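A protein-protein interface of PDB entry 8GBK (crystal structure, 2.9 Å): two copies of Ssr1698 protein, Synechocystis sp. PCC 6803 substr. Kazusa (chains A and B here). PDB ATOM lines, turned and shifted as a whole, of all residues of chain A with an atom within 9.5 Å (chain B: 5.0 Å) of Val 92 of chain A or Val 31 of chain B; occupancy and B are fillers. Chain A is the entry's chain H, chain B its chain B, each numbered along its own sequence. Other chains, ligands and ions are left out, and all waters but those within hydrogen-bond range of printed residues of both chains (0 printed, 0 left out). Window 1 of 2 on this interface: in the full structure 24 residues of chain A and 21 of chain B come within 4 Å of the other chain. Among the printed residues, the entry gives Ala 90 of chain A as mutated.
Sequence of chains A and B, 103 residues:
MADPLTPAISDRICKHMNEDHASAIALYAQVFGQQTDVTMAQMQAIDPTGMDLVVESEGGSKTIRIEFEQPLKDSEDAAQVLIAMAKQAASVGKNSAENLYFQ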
ATOM      1  N   LEU A  27      -9.283   5.499 -18.288  1.00  0.00           N
ATOM      2  CA  LEU A  27      -9.950   5.562 -16.992  1.00  0.00           C
ATOM      3  C   LEU A  27      -9.095   4.928 -15.904  1.00  0.00           C
ATOM      4  O   LEU A  27      -9.023   5.441 -14.782  1.00  0.00           O
ATOM      5  CB  LEU A  27     -11.311   4.875 -17.069  1.00  0.00           C
ATOM      6  CG  LEU A  27     -12.463   5.736 -17.587  1.00  0.00           C
ATOM      7  CD1 LEU A  27     -12.215   6.153 -19.031  1.00  0.00           C
ATOM      8  CD2 LEU A  27     -13.783   4.991 -17.457  1.00  0.00           C
ATOM      9  N   TYR A  28      -8.452   3.799 -16.210  1.00  0.00           N
ATOM     10  CA  TYR A  28      -7.586   3.162 -15.226  1.00  0.00           C
ATOM     11  C   TYR A  28      -6.495   4.122 -14.769  1.00  0.00           C
ATOM     12  O   TYR A  28      -6.271   4.304 -13.566  1.00  0.00           O
ATOM     13  CB  TYR A  28      -6.966   1.896 -15.816  1.00  0.00           C
ATOM     14  CG  TYR A  28      -7.955   0.836 -16.243  1.00  0.00           C
ATOM     15  CD1 TYR A  28      -9.189   0.708 -15.620  1.00  0.00           C
ATOM     16  CD2 TYR A  28      -7.647  -0.046 -17.272  1.00  0.00           C
ATOM     17  CE1 TYR A  28     -10.089  -0.269 -16.013  1.00  0.00           C
ATOM     18  CE2 TYR A  28      -8.538  -1.020 -17.671  1.00  0.00           C
ATOM     19  CZ  TYR A  28      -9.755  -1.130 -17.039  1.00  0.00           C
ATOM     20  OH  TYR A  28     -10.636  -2.106 -17.442  1.00  0.00           O
ATOM     21  N   ALA A  29      -5.822   4.769 -15.722  1.00  0.00           N
ATOM     22  CA  ALA A  29      -4.711   5.651 -15.377  1.00  0.00           C
ATOM     23  C   ALA A  29      -5.191   6.858 -14.582  1.00  0.00           C
ATOM     24  O   ALA A  29      -4.516   7.303 -13.646  1.00  0.00           O
ATOM     25  CB  ALA A  29      -3.983   6.099 -16.642  1.00  0.00           C
ATOM     26  N   GLN A  30      -6.355   7.397 -14.937  1.00  0.00           N
ATOM     27  CA  GLN A  30      -6.870   8.570 -14.244  1.00  0.00           C
ATOM     28  C   GLN A  30      -7.329   8.214 -12.839  1.00  0.00           C
ATOM     29  O   GLN A  30      -6.904   8.836 -11.858  1.00  0.00           O
ATOM     30  CB  GLN A  30      -8.022   9.174 -15.045  1.00  0.00           C
ATOM     31  CG  GLN A  30      -8.762  10.294 -14.345  1.00  0.00           C
ATOM     32  CD  GLN A  30     -10.016  10.690 -15.095  1.00  0.00           C
ATOM     33  OE1 GLN A  30     -10.873  11.392 -14.558  1.00  0.00           O
ATOM     34  NE2 GLN A  30     -10.121  10.267 -16.349  1.00  0.00           N
ATOM     35  N   VAL A  31      -8.188   7.203 -12.718  1.00  0.00           N
ATOM     36  CA  VAL A  31      -8.741   6.848 -11.414  1.00  0.00           C
ATOM     37  C   VAL A  31      -7.686   6.173 -10.551  1.00  0.00           C
ATOM     38  O   VAL A  31      -7.286   6.691  -9.501  1.00  0.00           O
ATOM     39  CB  VAL A  31      -9.978   5.949 -11.582  1.00  0.00           C
ATOM     40  CG1 VAL A  31     -10.449   5.447 -10.231  1.00  0.00           C
ATOM     41  CG2 VAL A  31     -11.092   6.705 -12.290  1.00  0.00           C
ATOM     42  N   PHE A  32      -7.209   5.010 -10.990  1.00  0.00           N
ATOM     43  CA  PHE A  32      -6.310   4.226 -10.151  1.00  0.00           C
ATOM     44  C   PHE A  32      -4.887   4.770 -10.159  1.00  0.00           C
ATOM     45  O   PHE A  32      -4.209   4.736  -9.129  1.00  0.00           O
ATOM     46  CB  PHE A  32      -6.335   2.766 -10.608  1.00  0.00           C
ATOM     47  CG  PHE A  32      -7.695   2.132 -10.504  1.00  0.00           C
ATOM     48  CD1 PHE A  32      -8.317   1.973  -9.275  1.00  0.00           C
ATOM     49  CD2 PHE A  32      -8.371   1.732 -11.643  1.00  0.00           C
ATOM     50  CE1 PHE A  32      -9.575   1.392  -9.188  1.00  0.00           C
ATOM     51  CE2 PHE A  32      -9.624   1.161 -11.563  1.00  0.00           C
ATOM     52  CZ  PHE A  32     -10.228   0.990 -10.338  1.00  0.00           C
ATOM     53  N   GLY A  33      -4.412   5.271 -11.292  1.00  0.00           N
ATOM     54  CA  GLY A  33      -3.070   5.816 -11.337  1.00  0.00           C
ATOM     55  C   GLY A  33      -2.948   7.306 -11.099  1.00  0.00           C
ATOM     56  O   GLY A  33      -1.940   7.915 -11.473  1.00  0.00           O
ATOM     57  N   GLN A  34      -4.000   7.883 -10.536  1.00  0.00           N
ATOM     58  CA  GLN A  34      -4.034   9.322 -10.173  1.00  0.00           C
ATOM     59  C   GLN A  34      -3.385  10.196 -11.243  1.00  0.00           C
ATOM     60  O   GLN A  34      -2.644  11.120 -10.885  1.00  0.00           O
ATOM     61  CB  GLN A  34      -3.483   9.493  -8.758  1.00  0.00           C
ATOM     62  CG  GLN A  34      -4.420   8.993  -7.673  1.00  0.00           C
ATOM     63  CD  GLN A  34      -3.774   7.936  -6.817  1.00  0.00           C
ATOM     64  OE1 GLN A  34      -2.578   7.973  -6.548  1.00  0.00           O
ATOM     65  NE2 GLN A  34      -4.571   6.980  -6.379  1.00  0.00           N
ATOM     66  N   GLN A  35      -3.700   9.934 -12.503  1.00  0.00           N
ATOM     67  CA  GLN A  35      -3.229  10.815 -13.596  1.00  0.00           C
ATOM     68  C   GLN A  35      -4.376  11.757 -13.949  1.00  0.00           C
ATOM     69  O   GLN A  35      -5.528  11.396 -13.762  1.00  0.00           O
ATOM     70  CB  GLN A  35      -2.741   9.993 -14.785  1.00  0.00           C
ATOM     71  CG  GLN A  35      -1.484   9.182 -14.516  1.00  0.00           C
ATOM     72  CD  GLN A  35      -0.229  10.011 -14.607  1.00  0.00           C
ATOM     73  OE1 GLN A  35       0.499  10.170 -13.637  1.00  0.00           O
ATOM     74  NE2 GLN A  35       0.035  10.545 -15.786  1.00  0.00           N
ATOM     75  N   THR A  36      -4.063  12.945 -14.425  1.00  0.00           N
ATOM     76  CA  THR A  36      -5.140  13.935 -14.637  1.00  0.00           C
ATOM     77  C   THR A  36      -5.349  14.125 -16.135  1.00  0.00           C
ATOM     78  O   THR A  36      -6.473  13.904 -16.613  1.00  0.00           O
ATOM     79  CB  THR A  36      -4.783  15.229 -13.895  1.00  0.00           C
ATOM     80  OG1 THR A  36      -4.798  14.971 -12.491  1.00  0.00           O
ATOM     81  CG2 THR A  36      -5.704  16.388 -14.206  1.00  0.00           C
ATOM     82  N   MET A  85     -13.198  -2.860 -12.931  1.00  0.00           N
ATOM     83  CA  MET A  85     -12.389  -1.683 -12.640  1.00  0.00           C
ATOM     84  C   MET A  85     -12.817  -0.498 -13.494  1.00  0.00           C
ATOM     85  O   MET A  85     -12.811   0.646 -13.027  1.00  0.00           O
ATOM     86  CB  MET A  85     -10.909  -2.000 -12.848  1.00  0.00           C
ATOM     87  CG  MET A  85     -10.268  -2.713 -11.666  1.00  0.00           C
ATOM     88  SD  MET A  85      -8.576  -3.251 -11.981  1.00  0.00           S
ATOM     89  CE  MET A  85      -7.813  -1.710 -12.479  1.00  0.00           C
ATOM     90  N   ALA A  86     -13.188  -0.749 -14.751  1.00  0.00           N
ATOM     91  CA  ALA A  86     -13.654   0.339 -15.603  1.00  0.00           C
ATOM     92  C   ALA A  86     -14.984   0.896 -15.110  1.00  0.00           C
ATOM     93  O   ALA A  86     -15.183   2.117 -15.092  1.00  0.00           O
ATOM     94  CB  ALA A  86     -13.776  -0.140 -17.046  1.00  0.00           C
ATOM     95  N   LYS A  87     -15.905   0.023 -14.692  1.00  0.00           N
ATOM     96  CA  LYS A  87     -17.182   0.503 -14.175  1.00  0.00           C
ATOM     97  C   LYS A  87     -16.992   1.308 -12.898  1.00  0.00           C
ATOM     98  O   LYS A  87     -17.596   2.373 -12.730  1.00  0.00           O
ATOM     99  CB  LYS A  87     -18.130  -0.670 -13.934  1.00  0.00           C
ATOM    100  CG  LYS A  87     -18.601  -1.356 -15.205  1.00  0.00           C
ATOM    101  CD  LYS A  87     -19.249  -2.696 -14.905  1.00  0.00           C
ATOM    102  CE  LYS A  87     -19.852  -3.313 -16.158  1.00  0.00           C
ATOM    103  NZ  LYS A  87     -20.432  -4.658 -15.889  1.00  0.00           N
ATOM    104  N   GLN A  88     -16.145   0.823 -11.989  1.00  0.00           N
ATOM    105  CA  GLN A  88     -15.876   1.571 -10.766  1.00  0.00           C
ATOM    106  C   GLN A  88     -15.224   2.910 -11.082  1.00  0.00           C
ATOM    107  O   GLN A  88     -15.517   3.920 -10.433  1.00  0.00           O
ATOM    108  CB  GLN A  88     -15.001   0.745  -9.824  1.00  0.00           C
ATOM    109  CG  GLN A  88     -14.681   1.438  -8.509  1.00  0.00           C
ATOM    110  CD  GLN A  88     -13.640   0.697  -7.695  1.00  0.00           C
ATOM    111  OE1 GLN A  88     -12.874  -0.107  -8.226  1.00  0.00           O
ATOM    112  NE2 GLN A  88     -13.611   0.960  -6.393  1.00  0.00           N
ATOM    113  N   ALA A  89     -14.340   2.936 -12.081  1.00  0.00           N
ATOM    114  CA  ALA A  89     -13.719   4.191 -12.486  1.00  0.00           C
ATOM    115  C   ALA A  89     -14.739   5.154 -13.078  1.00  0.00           C
ATOM    116  O   ALA A  89     -14.594   6.374 -12.937  1.00  0.00           O
ATOM    117  CB  ALA A  89     -12.597   3.924 -13.488  1.00  0.00           C
ATOM    118  N   ALA A  90     -15.775   4.630 -13.735  1.00  0.00           N
ATOM    119  CA  ALA A  90     -16.804   5.494 -14.304  1.00  0.00           C
ATOM    120  C   ALA A  90     -17.543   6.273 -13.224  1.00  0.00           C
ATOM    121  O   ALA A  90     -18.029   7.380 -13.480  1.00  0.00           O
ATOM    122  CB  ALA A  90     -17.788   4.666 -15.128  1.00  0.00           C
ATOM    123  N   SER A  91     -17.629   5.723 -12.011  1.00  0.00           N
ATOM    124  CA  SER A  91     -18.338   6.413 -10.938  1.00  0.00           C
ATOM    125  C   SER A  91     -17.534   7.599 -10.427  1.00  0.00           C
ATOM    126  O   SER A  91     -18.098   8.653 -10.112  1.00  0.00           O
ATOM    127  CB  SER A  91     -18.639   5.441  -9.800  1.00  0.00           C
ATOM    128  OG  SER A  91     -19.251   4.265 -10.296  1.00  0.00           O
ATOM    129  N   VAL A  92     -16.213   7.447 -10.333  1.00  0.00           N
ATOM    130  CA  VAL A  92     -15.376   8.559  -9.897  1.00  0.00           C
ATOM    131  C   VAL A  92     -15.450   9.693 -10.909  1.00  0.00           C
ATOM    132  O   VAL A  92     -15.519  10.873 -10.544  1.00  0.00           O
ATOM    133  CB  VAL A  92     -13.930   8.082  -9.668  1.00  0.00           C
ATOM    134  CG1 VAL A  92     -13.024   9.265  -9.368  1.00  0.00           C
ATOM    135  CG2 VAL A  92     -13.890   7.077  -8.533  1.00  0.00           C
ATOM    136  N   GLY A  93     -15.444   9.353 -12.198  1.00  0.00           N
ATOM    137  CA  GLY A  93     -15.534  10.359 -13.241  1.00  0.00           C
ATOM    138  C   GLY A  93     -16.758  11.239 -13.115  1.00  0.00           C
ATOM    139  O   GLY A  93     -16.758  12.367 -13.620  1.00  0.00           O
ATOM    140  N   LYS A  94     -17.798  10.756 -12.431  1.00  0.00           N
ATOM    141  CA  LYS A  94     -19.016  11.540 -12.280  1.00  0.00           C
ATOM    142  C   LYS A  94     -18.840  12.687 -11.300  1.00  0.00           C
ATOM    143  O   LYS A  94     -19.641  13.627 -11.321  1.00  0.00           O
ATOM    144  CB  LYS A  94     -20.169  10.665 -11.784  1.00  0.00           C
ATOM    145  CG  LYS A  94     -20.688   9.608 -12.734  1.00  0.00           C
ATOM    146  CD  LYS A  94     -21.362  10.240 -13.932  1.00  0.00           C
ATOM    147  CE  LYS A  94     -22.131   9.206 -14.727  1.00  0.00           C
ATOM    148  NZ  LYS A  94     -23.266   8.645 -13.943  1.00  0.00           N
ATOM    149  N   ASN A  95     -17.814  12.638 -10.452  1.00  0.00           N
ATOM    150  CA  ASN A  95     -17.486  13.736  -9.542  1.00  0.00           C
ATOM    151  C   ASN A  95     -16.287  14.468 -10.135  1.00  0.00           C
ATOM    152  O   ASN A  95     -15.134  14.117  -9.884  1.00  0.00           O
ATOM    153  CB  ASN A  95     -17.206  13.216  -8.137  1.00  0.00           C
ATOM    154  CG  ASN A  95     -18.422  12.579  -7.502  1.00  0.00           C
ATOM    155  OD1 ASN A  95     -19.210  13.250  -6.838  1.00  0.00           O
ATOM    156  ND2 ASN A  95     -18.586  11.277  -7.706  1.00  0.00           N
ATOM    157  N   SER A  96     -16.566  15.493 -10.933  1.00  0.00           N
ATOM    158  CA  SER A  96     -15.508  16.197 -11.643  1.00  0.00           C
ATOM    159  C   SER A  96     -14.588  16.922 -10.669  1.00  0.00           C
ATOM    160  O   SER A  96     -15.031  17.479  -9.661  1.00  0.00           O
ATOM    161  CB  SER A  96     -16.105  17.190 -12.642  1.00  0.00           C
ATOM    162  OG  SER A  96     -16.867  18.189 -11.987  1.00  0.00           O
ATOM    163  N   ALA A  97     -13.295  16.908 -10.977  1.00  0.00           N
ATOM    164  CA  ALA A  97     -12.289  17.636 -10.220  1.00  0.00           C
ATOM    165  C   ALA A  97     -11.797  18.810 -11.053  1.00  0.00           C
ATOM    166  O   ALA A  97     -11.371  18.629 -12.199  1.00  0.00           O
ATOM    167  CB  ALA A  97     -11.117  16.729  -9.844  1.00  0.00           C
ATOM    168  N   LEU B  27      -8.294  11.256   1.239  1.00  0.00           N
ATOM    169  CA  LEU B  27      -8.802  10.346   0.218  1.00  0.00           C
ATOM    170  C   LEU B  27      -9.517  11.106  -0.890  1.00  0.00           C
ATOM    171  O   LEU B  27      -9.359  10.787  -2.075  1.00  0.00           O
ATOM    172  CB  LEU B  27      -9.746   9.327   0.855  1.00  0.00           C
ATOM    173  CG  LEU B  27      -9.103   8.091   1.484  1.00  0.00           C
ATOM    174  CD1 LEU B  27      -8.218   8.489   2.656  1.00  0.00           C
ATOM    175  CD2 LEU B  27     -10.173   7.099   1.923  1.00  0.00           C
ATOM    176  N   TYR B  28     -10.310  12.112  -0.525  1.00  0.00           N
ATOM    177  CA  TYR B  28     -11.021  12.895  -1.530  1.00  0.00           C
ATOM    178  C   TYR B  28     -10.056  13.520  -2.530  1.00  0.00           C
ATOM    179  O   TYR B  28     -10.257  13.427  -3.746  1.00  0.00           O
ATOM    180  CB  TYR B  28     -11.864  13.975  -0.850  1.00  0.00           C
ATOM    181  CG  TYR B  28     -12.952  13.448   0.060  1.00  0.00           C
ATOM    182  CD1 TYR B  28     -13.548  12.216  -0.176  1.00  0.00           C
ATOM    183  CD2 TYR B  28     -13.396  14.191   1.145  1.00  0.00           C
ATOM    184  CE1 TYR B  28     -14.551  11.736   0.648  1.00  0.00           C
ATOM    185  CE2 TYR B  28     -14.396  13.719   1.974  1.00  0.00           C
ATOM    186  CZ  TYR B  28     -14.970  12.491   1.720  1.00  0.00           C
ATOM    187  OH  TYR B  28     -15.969  12.018   2.541  1.00  0.00           O
ATOM    188  N   ALA B  29      -8.984  14.140  -2.036  1.00  0.00           N
ATOM    189  CA  ALA B  29      -8.084  14.862  -2.929  1.00  0.00           C
ATOM    190  C   ALA B  29      -7.394  13.925  -3.909  1.00  0.00           C
ATOM    191  O   ALA B  29      -7.241  14.255  -5.091  1.00  0.00           O
ATOM    192  CB  ALA B  29      -7.052  15.640  -2.115  1.00  0.00           C
ATOM    193  N   GLN B  30      -6.978  12.746  -3.447  1.00  0.00           N
ATOM    194  CA  GLN B  30      -6.280  11.823  -4.335  1.00  0.00           C
ATOM    195  C   GLN B  30      -7.242  11.189  -5.330  1.00  0.00           C
ATOM    196  O   GLN B  30      -7.010  11.227  -6.544  1.00  0.00           O
ATOM    197  CB  GLN B  30      -5.549  10.755  -3.520  1.00  0.00           C
ATOM    198  CG  GLN B  30      -4.277  11.257  -2.848  1.00  0.00           C
ATOM    199  CD  GLN B  30      -3.506  10.151  -2.155  1.00  0.00           C
ATOM    200  OE1 GLN B  30      -4.042   9.076  -1.891  1.00  0.00           O
ATOM    201  NE2 GLN B  30      -2.236  10.410  -1.861  1.00  0.00           N
ATOM    202  N   VAL B  31      -8.338  10.611  -4.838  1.00  0.00           N
ATOM    203  CA  VAL B  31      -9.269   9.916  -5.723  1.00  0.00           C
ATOM    204  C   VAL B  31     -10.050  10.915  -6.566  1.00  0.00           C
ATOM    205  O   VAL B  31      -9.929  10.950  -7.797  1.00  0.00           O
ATOM    206  CB  VAL B  31     -10.212   9.015  -4.908  1.00  0.00           C
ATOM    207  CG1 VAL B  31     -11.278   8.412  -5.806  1.00  0.00           C
ATOM    208  CG2 VAL B  31      -9.425   7.923  -4.198  1.00  0.00           C
ATOM    209  N   PHE B  32     -10.854  11.753  -5.913  1.00  0.00           N
ATOM    210  CA  PHE B  32     -11.726  12.671  -6.637  1.00  0.00           C
ATOM    211  C   PHE B  32     -10.982  13.887  -7.173  1.00  0.00           C
ATOM    212  O   PHE B  32     -11.336  14.398  -8.240  1.00  0.00           O
ATOM    213  CB  PHE B  32     -12.893  13.100  -5.745  1.00  0.00           C
ATOM    214  CG  PHE B  32     -13.798  11.963  -5.354  1.00  0.00           C
ATOM    215  CD1 PHE B  32     -14.514  11.265  -6.320  1.00  0.00           C
ATOM    216  CD2 PHE B  32     -13.920  11.577  -4.034  1.00  0.00           C
ATOM    217  CE1 PHE B  32     -15.351  10.218  -5.963  1.00  0.00           C
ATOM    218  CE2 PHE B  32     -14.748  10.532  -3.672  1.00  0.00           C
ATOM    219  CZ  PHE B  32     -15.464   9.851  -4.636  1.00  0.00           C
ATOM    220  N   GLY B  33      -9.958  14.361  -6.468  1.00  0.00           N
ATOM    221  CA  GLY B  33      -9.212  15.507  -6.947  1.00  0.00           C
ATOM    222  C   GLY B  33      -8.054  15.193  -7.860  1.00  0.00           C
ATOM    223  O   GLY B  33      -7.505  16.103  -8.489  1.00  0.00           O
ATOM    224  N   GLN B  34      -7.681  13.920  -7.964  1.00  0.00           N
ATOM    225  CA  GLN B  34      -6.624  13.472  -8.869  1.00  0.00           C
ATOM    226  C   GLN B  34      -5.274  14.087  -8.524  1.00  0.00           C
ATOM    227  O   GLN B  34      -4.424  14.273  -9.399  1.00  0.00           O
ATOM    228  CB  GLN B  34      -6.976  13.812 -10.317  1.00  0.00           C
ATOM    229  CG  GLN B  34      -8.111  13.013 -10.905  1.00  0.00           C
ATOM    230  CD  GLN B  34      -8.514  13.536 -12.268  1.00  0.00           C
ATOM    231  OE1 GLN B  34      -7.774  14.290 -12.900  1.00  0.00           O
ATOM    232  NE2 GLN B  34      -9.706  13.167 -12.712  1.00  0.00           N
ATOM    233  N   GLN B  88     -16.077   5.046  -1.444  1.00  0.00           N
ATOM    234  CA  GLN B  88     -15.665   4.847  -2.852  1.00  0.00           C
ATOM    235  C   GLN B  88     -14.175   5.126  -2.937  1.00  0.00           C
ATOM    236  O   GLN B  88     -13.513   4.527  -3.776  1.00  0.00           O
ATOM    237  CB  GLN B  88     -16.429   5.823  -3.735  1.00  0.00           C
ATOM    238  CG  GLN B  88     -16.344   5.550  -5.225  1.00  0.00           C
ATOM    239  CD  GLN B  88     -17.105   6.607  -5.985  1.00  0.00           C
ATOM    240  OE1 GLN B  88     -16.568   7.281  -6.856  1.00  0.00           O
ATOM    241  NE2 GLN B  88     -18.372   6.774  -5.644  1.00  0.00           N
ATOM    242  N   ALA B  89     -13.678   6.003  -2.078  1.00  0.00           N
ATOM    243  CA  ALA B  89     -12.254   6.373  -2.114  1.00  0.00           C
ATOM    244  C   ALA B  89     -11.426   5.295  -1.429  1.00  0.00           C
ATOM    245  O   ALA B  89     -10.269   5.127  -1.803  1.00  0.00           O
ATOM    246  CB  ALA B  89     -12.100   7.693  -1.435  1.00  0.00           C
ATOM    247  N   VAL B  92     -11.269   2.437  -4.023  1.00  0.00           N
ATOM    248  CA  VAL B  92     -10.357   2.728  -5.160  1.00  0.00           C
ATOM    249  C   VAL B  92      -8.923   2.745  -4.650  1.00  0.00           C
ATOM    250  O   VAL B  92      -8.054   2.219  -5.345  1.00  0.00           O
ATOM    251  CB  VAL B  92     -10.734   4.042  -5.857  1.00  0.00           C
ATOM    252  CG1 VAL B  92      -9.612   4.562  -6.740  1.00  0.00           C
ATOM    253  CG2 VAL B  92     -12.016   3.896  -6.657  1.00  0.00           C
ATOM    254  N   GLY B  93      -8.687   3.314  -3.478  1.00  0.00           N
ATOM    255  CA  GLY B  93      -7.309   3.449  -2.981  1.00  0.00           C
ATOM    256  C   GLY B  93      -6.666   2.105  -2.756  1.00  0.00           C
ATOM    257  O   GLY B  93      -5.440   2.024  -2.821  1.00  0.00           O
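Of the printed residues of chain B, Gln 35 of chain A touches Gln 34 (3.8 Å). Printed residues of chain B within 4 Å of Gln 88 of chain A: Val 92 (3.4 Å). Val 92 of chain A touches three residues of chain B. Of chain A, only Val 92 comes within 4 Å of Val 31 of chain B. No residue of chain A comes within 4 Å of Ala 89 of chain B. The nearest residue of chain B that does not touch Val 92 of chain A is Val 92 of chain B (4.1 Å). The nearest printed residue of chain B that does not touch Phe 32 of chain A is Gly 93 of chain B (6.0 Å).
Val 31 of chain A touches Val 92 of chain B, and with the chains exchanged Val 92 of chain A touches Val 31 of chain B. Phe 32 of chain A touches Val 92 of chain B, and with the chains exchanged Val 92 of chain A touches Phe 32 of chain B. Gln 34 of chain B touches its own counterpart, Gln 34 of chain A. Gln 88 of chain A touches Val 92 of chain B, and with the chains exchanged Val 92 of chain A touches Gln 88 of chain B. Positions printed for both chains: 27, 28, 29, 30, 31, 32, 33, 34, 88, 89, 92 and 93. Of the 15 pairs that touch across the chains among the printed residues, 9 have their exchanged pair printed and touching as well.
Of the 12 printed residues of chain B, 7 touch a printed residue of chain A. Printed residues of chain B that touch a printed residue of chain A: Gln 30, Val 31, Phe 32, Gly 33, Gln 34, Gln 88 and Val 92. Hydrophobic or aromatic side chains of chain B within 4 Å of the printed part of chain A: Phe 32 and Val 92. Among the printed residues, 15 pairs touch across the chains. Among the printed residues, no Asp or Glu carboxylate lies within 4 Å of a Lys or Arg side-chain nitrogen of the other chain.
N of Gly 33 of chain B lies within hydrogen-bond range of O of Tyr 28 of chain B (2.9 Å). O of Ala 29 of chain B is in hydrogen-bond range of N of Gln 34 of chain B (2.9 Å). The side-chain hydroxyl (OG) of Ser 91 of chain A sits at hydrogen-bond distance from the backbone carbonyl oxygen (O) of Lys 87 of chain A, 3.5 Å away. N of Gln 35 of chain A lies within hydrogen-bond range of O of Ala 29 of chain A, 3.0 Å away. The backbone carbonyl oxygen of Ala 29 of chain A sits at hydrogen-bond distance from the backbone NH of Gln 34 of chain A (3.2 Å). O of Gln 30 of chain A is in hydrogen-bond range of N of Gln 35 of chain A.
Phe 32 of chain A touches Val 92 of chain B. Gln 34 of chain A touches Gln 30 of chain B. Gln 34 of chain A touches Gln 34 of chain B. O of Gln 35 of chain A touches OE1 of Gln 34 of chain B, at 3.8 Å. Ser 91 of chain A touches Gln 88 of chain B (C to OE1, 3.7 Å). Val 92 of chain A touches Val 31 of chain B (CG1 to O, 3.9 Å). CD1 of Phe 32 of chain B touches CG1 of Val 92 of chain A, at 3.9 Å. Asn 95 of chain A touches Phe 32 of chain B. O of Phe 32 of chain B touches CB of Ala 97 of chain A, at 2.8 Å. Gly 33 of chain B touches Ala 97 of chain A.
OE1 of Gln 30 of chain A is in hydrogen-bond range of NE2 of Gln 34 of chain B (2.8 Å). OG1 of Thr 36 of chain A sits at hydrogen-bond distance from OE1 of Gln 34 of chain B, at 3.1 Å. The backbone NH (N) of Val 92 of chain A lies close to the side-chain amide oxygen (OE1) of Gln 88 of chain B, 3.5 Å away.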
